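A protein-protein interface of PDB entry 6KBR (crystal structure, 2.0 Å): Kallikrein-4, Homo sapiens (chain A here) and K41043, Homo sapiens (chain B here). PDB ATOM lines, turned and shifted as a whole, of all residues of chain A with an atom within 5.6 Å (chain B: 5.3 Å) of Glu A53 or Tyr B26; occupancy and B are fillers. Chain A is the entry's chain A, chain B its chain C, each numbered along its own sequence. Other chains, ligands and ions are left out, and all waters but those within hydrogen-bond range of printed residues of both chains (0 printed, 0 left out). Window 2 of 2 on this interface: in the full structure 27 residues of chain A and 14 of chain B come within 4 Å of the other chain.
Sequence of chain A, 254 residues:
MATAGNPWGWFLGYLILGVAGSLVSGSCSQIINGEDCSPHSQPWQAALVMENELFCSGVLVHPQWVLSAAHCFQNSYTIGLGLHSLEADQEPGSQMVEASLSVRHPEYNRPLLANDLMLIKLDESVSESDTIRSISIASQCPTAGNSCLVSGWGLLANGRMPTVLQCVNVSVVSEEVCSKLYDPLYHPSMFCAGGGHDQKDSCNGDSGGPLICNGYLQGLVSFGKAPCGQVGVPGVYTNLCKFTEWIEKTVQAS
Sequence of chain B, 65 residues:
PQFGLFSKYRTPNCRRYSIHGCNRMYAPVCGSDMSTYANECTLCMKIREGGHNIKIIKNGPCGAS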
ATOM      1  N   LEU A  48      -2.872  -2.009  -9.895  1.00  0.00           N
ATOM      2  CA  LEU A  48      -1.793  -1.061  -9.450  1.00  0.00           C
ATOM      3  C   LEU A  48      -2.326   0.359  -9.735  1.00  0.00           C
ATOM      4  O   LEU A  48      -2.563   0.722 -10.872  1.00  0.00           O
ATOM      5  CB  LEU A  48      -0.457  -1.333 -10.179  1.00  0.00           C
ATOM      6  CG  LEU A  48       0.431  -2.440  -9.538  1.00  0.00           C
ATOM      7  CD1 LEU A  48      -0.222  -3.739  -9.139  1.00  0.00           C
ATOM      8  CD2 LEU A  48       1.638  -2.771 -10.429  1.00  0.00           C
ATOM      9  N   VAL A  49      -2.477   1.145  -8.698  1.00  0.00           N
ATOM     10  CA  VAL A  49      -3.101   2.451  -8.763  1.00  0.00           C
ATOM     11  C   VAL A  49      -2.159   3.492  -8.107  1.00  0.00           C
ATOM     12  O   VAL A  49      -1.393   3.178  -7.176  1.00  0.00           O
ATOM     13  CB  VAL A  49      -4.470   2.440  -8.056  1.00  0.00           C
ATOM     14  CG1 VAL A  49      -5.463   1.538  -8.764  1.00  0.00           C
ATOM     15  CG2 VAL A  49      -4.328   1.836  -6.667  1.00  0.00           C
ATOM     16  N   MET A  50      -2.197   4.717  -8.617  1.00  0.00           N
ATOM     17  CA  MET A  50      -1.563   5.884  -7.953  1.00  0.00           C
ATOM     18  C   MET A  50      -2.340   7.094  -8.409  1.00  0.00           C
ATOM     19  O   MET A  50      -2.846   7.111  -9.556  1.00  0.00           O
ATOM     20  CB  MET A  50      -0.092   6.003  -8.314  1.00  0.00           C
ATOM     21  CG  MET A  50       0.273   6.329  -9.766  1.00  0.00           C
ATOM     22  SD  MET A  50       2.095   6.178 -10.103  1.00  0.00           S
ATOM     23  CE  MET A  50       1.838   6.193 -11.880  1.00  0.00           C
ATOM     24  N   GLU A  51      -2.459   8.078  -7.534  1.00  0.00           N
ATOM     25  CA  GLU A  51      -3.328   9.255  -7.788  1.00  0.00           C
ATOM     26  C   GLU A  51      -4.748   8.791  -8.174  1.00  0.00           C
ATOM     27  O   GLU A  51      -5.312   9.300  -9.111  1.00  0.00           O
ATOM     28  CB  GLU A  51      -2.759  10.143  -8.934  1.00  0.00           C
ATOM     29  CG  GLU A  51      -1.251  10.423  -8.932  1.00  0.00           C
ATOM     30  CD  GLU A  51      -0.721  10.841  -7.576  1.00  0.00           C
ATOM     31  OE1 GLU A  51      -1.421  11.628  -6.867  1.00  0.00           O
ATOM     32  OE2 GLU A  51       0.398  10.361  -7.217  1.00  0.00           O
ATOM     33  N   ASN A  52      -5.276   7.760  -7.521  1.00  0.00           N
ATOM     34  CA  ASN A  52      -6.605   7.198  -7.855  1.00  0.00           C
ATOM     35  C   ASN A  52      -6.828   6.807  -9.364  1.00  0.00           C
ATOM     36  O   ASN A  52      -7.996   6.740  -9.830  1.00  0.00           O
ATOM     37  CB  ASN A  52      -7.693   8.186  -7.376  1.00  0.00           C
ATOM     38  CG  ASN A  52      -7.398   8.722  -5.983  1.00  0.00           C
ATOM     39  OD1 ASN A  52      -7.165   9.921  -5.785  1.00  0.00           O
ATOM     40  ND2 ASN A  52      -7.337   7.817  -5.013  1.00  0.00           N
ATOM     41  N   GLU A  53      -5.724   6.536 -10.085  1.00  0.00           N
ATOM     42  CA  GLU A  53      -5.716   6.162 -11.533  1.00  0.00           C
ATOM     43  C   GLU A  53      -4.914   4.822 -11.668  1.00  0.00           C
ATOM     44  O   GLU A  53      -3.790   4.697 -11.237  1.00  0.00           O
ATOM     45  CB  GLU A  53      -5.158   7.304 -12.378  1.00  0.00           C
ATOM     46  CG  GLU A  53      -5.076   7.157 -13.913  1.00  0.00           C
ATOM     47  CD  GLU A  53      -4.593   8.465 -14.693  1.00  0.00           C
ATOM     48  OE1 GLU A  53      -3.332   8.721 -14.869  1.00  0.00           O
ATOM     49  OE2 GLU A  53      -5.486   9.255 -15.227  1.00  0.00           O
ATOM     50  N   LEU A  54      -5.576   3.798 -12.192  1.00  0.00           N
ATOM     51  CA  LEU A  54      -4.963   2.548 -12.550  1.00  0.00           C
ATOM     52  C   LEU A  54      -3.957   2.724 -13.718  1.00  0.00           C
ATOM     53  O   LEU A  54      -4.334   3.263 -14.743  1.00  0.00           O
ATOM     54  CB  LEU A  54      -6.029   1.565 -13.021  1.00  0.00           C
ATOM     55  CG  LEU A  54      -5.459   0.149 -13.239  1.00  0.00           C
ATOM     56  CD1 LEU A  54      -6.344  -0.855 -12.566  1.00  0.00           C
ATOM     57  CD2 LEU A  54      -5.271  -0.169 -14.705  1.00  0.00           C
ATOM     58  N   PHE A  55      -2.721   2.251 -13.542  1.00  0.00           N
ATOM     59  CA  PHE A  55      -1.690   2.319 -14.597  1.00  0.00           C
ATOM     60  C   PHE A  55      -1.281   0.945 -15.140  1.00  0.00           C
ATOM     61  O   PHE A  55      -0.926   0.827 -16.326  1.00  0.00           O
ATOM     62  CB  PHE A  55      -0.478   3.152 -14.130  1.00  0.00           C
ATOM     63  CG  PHE A  55       0.218   2.630 -12.920  1.00  0.00           C
ATOM     64  CD1 PHE A  55      -0.199   3.003 -11.657  1.00  0.00           C
ATOM     65  CD2 PHE A  55       1.352   1.781 -13.047  1.00  0.00           C
ATOM     66  CE1 PHE A  55       0.438   2.538 -10.535  1.00  0.00           C
ATOM     67  CE2 PHE A  55       1.972   1.281 -11.919  1.00  0.00           C
ATOM     68  CZ  PHE A  55       1.528   1.693 -10.662  1.00  0.00           C
ATOM     69  N   CYS A  56      -1.399  -0.082 -14.282  1.00  0.00           N
ATOM     70  CA  CYS A  56      -1.089  -1.445 -14.623  1.00  0.00           C
ATOM     71  C   CYS A  56      -1.902  -2.374 -13.710  1.00  0.00           C
ATOM     72  O   CYS A  56      -2.514  -1.947 -12.730  1.00  0.00           O
ATOM     73  CB  CYS A  56       0.400  -1.709 -14.362  1.00  0.00           C
ATOM     74  SG  CYS A  56       1.571  -1.068 -15.581  1.00  0.00           S
ATOM     75  N   LEU A 155      -7.969  -0.138 -21.604  1.00  0.00           N
ATOM     76  CA  LEU A 155      -8.896   0.517 -22.497  1.00  0.00           C
ATOM     77  C   LEU A 155      -9.648  -0.537 -23.347  1.00  0.00           C
ATOM     78  O   LEU A 155      -9.124  -1.647 -23.644  1.00  0.00           O
ATOM     79  CB  LEU A 155      -8.195   1.547 -23.375  1.00  0.00           C
ATOM     80  CG  LEU A 155      -7.403   2.655 -22.651  1.00  0.00           C
ATOM     81  CD1 LEU A 155      -6.782   3.587 -23.691  1.00  0.00           C
ATOM     82  CD2 LEU A 155      -8.262   3.457 -21.688  1.00  0.00           C
ATOM     83  N   MET A 161     -12.770   3.590 -20.638  1.00  0.00           N
ATOM     84  CA  MET A 161     -12.367   2.612 -19.560  1.00  0.00           C
ATOM     85  C   MET A 161     -13.572   1.834 -19.089  1.00  0.00           C
ATOM     86  O   MET A 161     -14.603   2.401 -18.979  1.00  0.00           O
ATOM     87  CB  MET A 161     -11.760   3.340 -18.341  1.00  0.00           C
ATOM     88  CG  MET A 161     -10.984   4.615 -18.698  1.00  0.00           C
ATOM     89  SD  MET A 161      -9.945   5.250 -17.344  1.00  0.00           S
ATOM     90  CE  MET A 161      -8.627   4.133 -17.726  1.00  0.00           C
ATOM     91  N   ASN A 204      -3.716  -0.933 -23.579  1.00  0.00           N
ATOM     92  CA  ASN A 204      -3.086  -0.075 -22.612  1.00  0.00           C
ATOM     93  C   ASN A 204      -3.872  -0.034 -21.328  1.00  0.00           C
ATOM     94  O   ASN A 204      -5.103  -0.007 -21.373  1.00  0.00           O
ATOM     95  CB  ASN A 204      -2.883   1.307 -23.204  1.00  0.00           C
ATOM     96  CG  ASN A 204      -1.946   1.232 -24.406  1.00  0.00           C
ATOM     97  OD1 ASN A 204      -0.829   0.774 -24.266  1.00  0.00           O
ATOM     98  ND2 ASN A 204      -2.412   1.575 -25.561  1.00  0.00           N
ATOM     99  N   GLY A 205      -3.171  -0.051 -20.207  1.00  0.00           N
ATOM    100  CA  GLY A 205      -3.775  -0.304 -18.885  1.00  0.00           C
ATOM    101  C   GLY A 205      -3.872  -1.764 -18.441  1.00  0.00           C
ATOM    102  O   GLY A 205      -4.075  -2.024 -17.263  1.00  0.00           O
ATOM    103  N   ARG B  24       2.179  -1.612 -22.528  1.00  0.00           N
ATOM    104  CA  ARG B  24       0.759  -1.432 -22.350  1.00  0.00           C
ATOM    105  C   ARG B  24       0.397  -0.853 -20.966  1.00  0.00           C
ATOM    106  O   ARG B  24      -0.660  -1.175 -20.398  1.00  0.00           O
ATOM    107  CB  ARG B  24       0.062  -2.760 -22.663  1.00  0.00           C
ATOM    108  CG  ARG B  24      -0.141  -2.849 -24.171  1.00  0.00           C
ATOM    109  CD  ARG B  24      -0.512  -4.220 -24.675  1.00  0.00           C
ATOM    110  NE  ARG B  24      -0.903  -4.124 -26.110  1.00  0.00           N
ATOM    111  CZ  ARG B  24      -1.520  -5.092 -26.793  1.00  0.00           C
ATOM    112  NH1 ARG B  24      -1.930  -6.234 -26.211  1.00  0.00           N
ATOM    113  NH2 ARG B  24      -1.752  -4.892 -28.072  1.00  0.00           N
ATOM    114  N   MET B  25       1.288  -0.001 -20.443  1.00  0.00           N
ATOM    115  CA  MET B  25       1.003   0.734 -19.219  1.00  0.00           C
ATOM    116  C   MET B  25       0.140   1.932 -19.592  1.00  0.00           C
ATOM    117  O   MET B  25       0.263   2.474 -20.682  1.00  0.00           O
ATOM    118  CB  MET B  25       2.292   1.194 -18.530  1.00  0.00           C
ATOM    119  CG  MET B  25       2.084   2.149 -17.386  1.00  0.00           C
ATOM    120  SD  MET B  25       3.647   2.357 -16.515  1.00  0.00           S
ATOM    121  CE  MET B  25       3.348   3.864 -15.550  1.00  0.00           C
ATOM    122  N   TYR B  26      -0.767   2.310 -18.715  1.00  0.00           N
ATOM    123  CA  TYR B  26      -1.595   3.509 -18.923  1.00  0.00           C
ATOM    124  C   TYR B  26      -0.903   4.683 -18.208  1.00  0.00           C
ATOM    125  O   TYR B  26      -0.852   4.692 -17.027  1.00  0.00           O
ATOM    126  CB  TYR B  26      -3.024   3.295 -18.429  1.00  0.00           C
ATOM    127  CG  TYR B  26      -3.942   4.493 -18.751  1.00  0.00           C
ATOM    128  CD1 TYR B  26      -4.336   4.777 -20.055  1.00  0.00           C
ATOM    129  CD2 TYR B  26      -4.420   5.327 -17.725  1.00  0.00           C
ATOM    130  CE1 TYR B  26      -5.182   5.859 -20.325  1.00  0.00           C
ATOM    131  CE2 TYR B  26      -5.254   6.409 -17.991  1.00  0.00           C
ATOM    132  CZ  TYR B  26      -5.628   6.662 -19.272  1.00  0.00           C
ATOM    133  OH  TYR B  26      -6.432   7.739 -19.501  1.00  0.00           O
ATOM    134  N   ALA B  27      -0.302   5.587 -18.987  1.00  0.00           N
ATOM    135  CA  ALA B  27       0.358   6.817 -18.536  1.00  0.00           C
ATOM    136  C   ALA B  27      -0.018   7.943 -19.513  1.00  0.00           C
ATOM    137  O   ALA B  27       0.795   8.350 -20.328  1.00  0.00           O
ATOM    138  CB  ALA B  27       1.879   6.624 -18.508  1.00  0.00           C
ATOM    139  N   PRO B  28      -1.264   8.443 -19.412  1.00  0.00           N
ATOM    140  CA  PRO B  28      -1.797   9.266 -20.500  1.00  0.00           C
ATOM    141  C   PRO B  28      -1.125  10.647 -20.710  1.00  0.00           C
ATOM    142  O   PRO B  28      -0.595  11.282 -19.757  1.00  0.00           O
ATOM    143  CB  PRO B  28      -3.308   9.358 -20.164  1.00  0.00           C
ATOM    144  CG  PRO B  28      -3.310   9.271 -18.630  1.00  0.00           C
ATOM    145  CD  PRO B  28      -2.260   8.250 -18.325  1.00  0.00           C
ATOM    146  N   THR B  36      -6.439  12.220 -26.253  1.00  0.00           N
ATOM    147  CA  THR B  36      -5.593  11.708 -25.151  1.00  0.00           C
ATOM    148  C   THR B  36      -4.958  10.397 -25.698  1.00  0.00           C
ATOM    149  O   THR B  36      -5.629   9.618 -26.314  1.00  0.00           O
ATOM    150  CB  THR B  36      -6.301  11.716 -23.732  1.00  0.00           C
ATOM    151  OG1 THR B  36      -6.033  10.522 -22.936  1.00  0.00           O
ATOM    152  CG2 THR B  36      -7.671  11.929 -23.818  1.00  0.00           C
ATOM    153  N   ALA B  38      -2.875   6.933 -24.766  1.00  0.00           N
ATOM    154  CA  ALA B  38      -2.656   6.025 -23.611  1.00  0.00           C
ATOM    155  C   ALA B  38      -1.248   6.146 -22.969  1.00  0.00           C
ATOM    156  O   ALA B  38      -1.080   5.992 -21.783  1.00  0.00           O
ATOM    157  CB  ALA B  38      -2.938   4.572 -23.984  1.00  0.00           C
ATOM    158  N   ASN B  39      -0.263   6.415 -23.779  1.00  0.00           N
ATOM    159  CA  ASN B  39       1.056   6.712 -23.310  1.00  0.00           C
ATOM    160  C   ASN B  39       1.838   7.428 -24.392  1.00  0.00           C
ATOM    161  O   ASN B  39       1.370   7.524 -25.511  1.00  0.00           O
ATOM    162  CB  ASN B  39       1.768   5.440 -22.837  1.00  0.00           C
ATOM    163  CG  ASN B  39       1.669   4.300 -23.832  1.00  0.00           C
ATOM    164  OD1 ASN B  39       1.933   4.464 -25.030  1.00  0.00           O
ATOM    165  ND2 ASN B  39       1.336   3.126 -23.334  1.00  0.00           N
ATOM    166  N   PRO B  61      -4.942  13.030 -19.031  1.00  0.00           N
ATOM    167  CA  PRO B  61      -5.916  13.068 -20.106  1.00  0.00           C
ATOM    168  C   PRO B  61      -6.140  14.509 -20.574  1.00  0.00           C
ATOM    169  O   PRO B  61      -5.760  15.445 -19.872  1.00  0.00           O
ATOM    170  CB  PRO B  61      -7.187  12.427 -19.494  1.00  0.00           C
ATOM    171  CG  PRO B  61      -6.972  12.392 -18.023  1.00  0.00           C
ATOM    172  CD  PRO B  61      -5.503  12.542 -17.744  1.00  0.00           C
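The backbone NH (N) of Tyr B26 lies within hydrogen-bond range of the backbone carbonyl oxygen (O) of Phe A55.
ND2 of Asn B39 sits at hydrogen-bond distance from OD1 of Asn A204, at 3.3 Å.
The backbone NH of Gly A205 lies within hydrogen-bond range of the backbone carbonyl oxygen of Arg B24, at 2.8 Å.
The backbone NH of Phe A55 sits at hydrogen-bond distance from the backbone carbonyl oxygen of Leu A48 (3.1 Å).
O of Cys A56 sits at hydrogen-bond distance from N of Leu A48 (2.9 Å).
The backbone NH (N) of Leu A155 is in hydrogen-bond range of the backbone carbonyl oxygen (O) of Asn A204.
The backbone carbonyl oxygen of Met B25 sits at hydrogen-bond distance from the side-chain amide nitrogen of Asn B39, at 2.9 Å.
O of Ala B38 is in hydrogen-bond range of N of Ala B27 (2.9 Å).
Tyr B26 touches Glu A53.
Glu A53 touches Pro B28.
O of Leu A54 touches CD2 of Tyr B26, at 3.6 Å.
Phe A55 touches Met B25.
Cys A56 touches Met B25 (SG to CG, 3.7 Å).
Leu A155 touches Ala B38.
Asn A204 touches Arg B24.
Asn A204 touches Ala B38 (CB to CB, 3.4 Å).
Met B25 touches Gly A205 (C to N, 3.9 Å).
N of Gly A205 touches N of Tyr B26 (3.7 Å).
Glu A53 touches just these residues of chain B: Tyr B26 (3.9 Å) and Pro B28 (3.6 Å).
Of chain A, only Glu A53 (3.9 Å), Leu A54 (3.6 Å), Phe A55 (2.8 Å) and Gly A205 (3.7 Å) come within 4 Å of Tyr B26.
Printed residues of chain A within 4 Å of Ala B38: Leu A155 and Asn A204.
Of the printed residues of chain B, Phe A55 touches Met B25 (3.5 Å) and Tyr B26 (2.8 Å).
Of the printed residues of chain A, Asn B39 touches Asn A204 (3.3 Å).
Of the printed residues of chain A, Met B25 touches Phe A55, Cys A56 and Gly A205.
Of the printed residues of chain B, Leu A54 touches Tyr B26 (3.6 Å).
Asn A52 touches none of the printed residues of chain B.
Leu A48 touches none of the printed residues of chain B.
Printed residues of chain A that touch a printed residue of chain B: Glu A53, Leu A54, Phe A55, Cys A56, Leu A155, Asn A204 and Gly A205.
Hydrophobic or aromatic side chains of chain A within 4 Å of the printed part of chain B: Phe A55 and Leu A155.
Of the 9 printed residues of chain B, 6 touch a printed residue of chain A.
Among the printed residues, 13 pairs touch across the chains.
Among the printed residues, no Asp or Glu carboxylate lies within 4 Å of a Lys or Arg side-chain nitrogen of the other chain.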
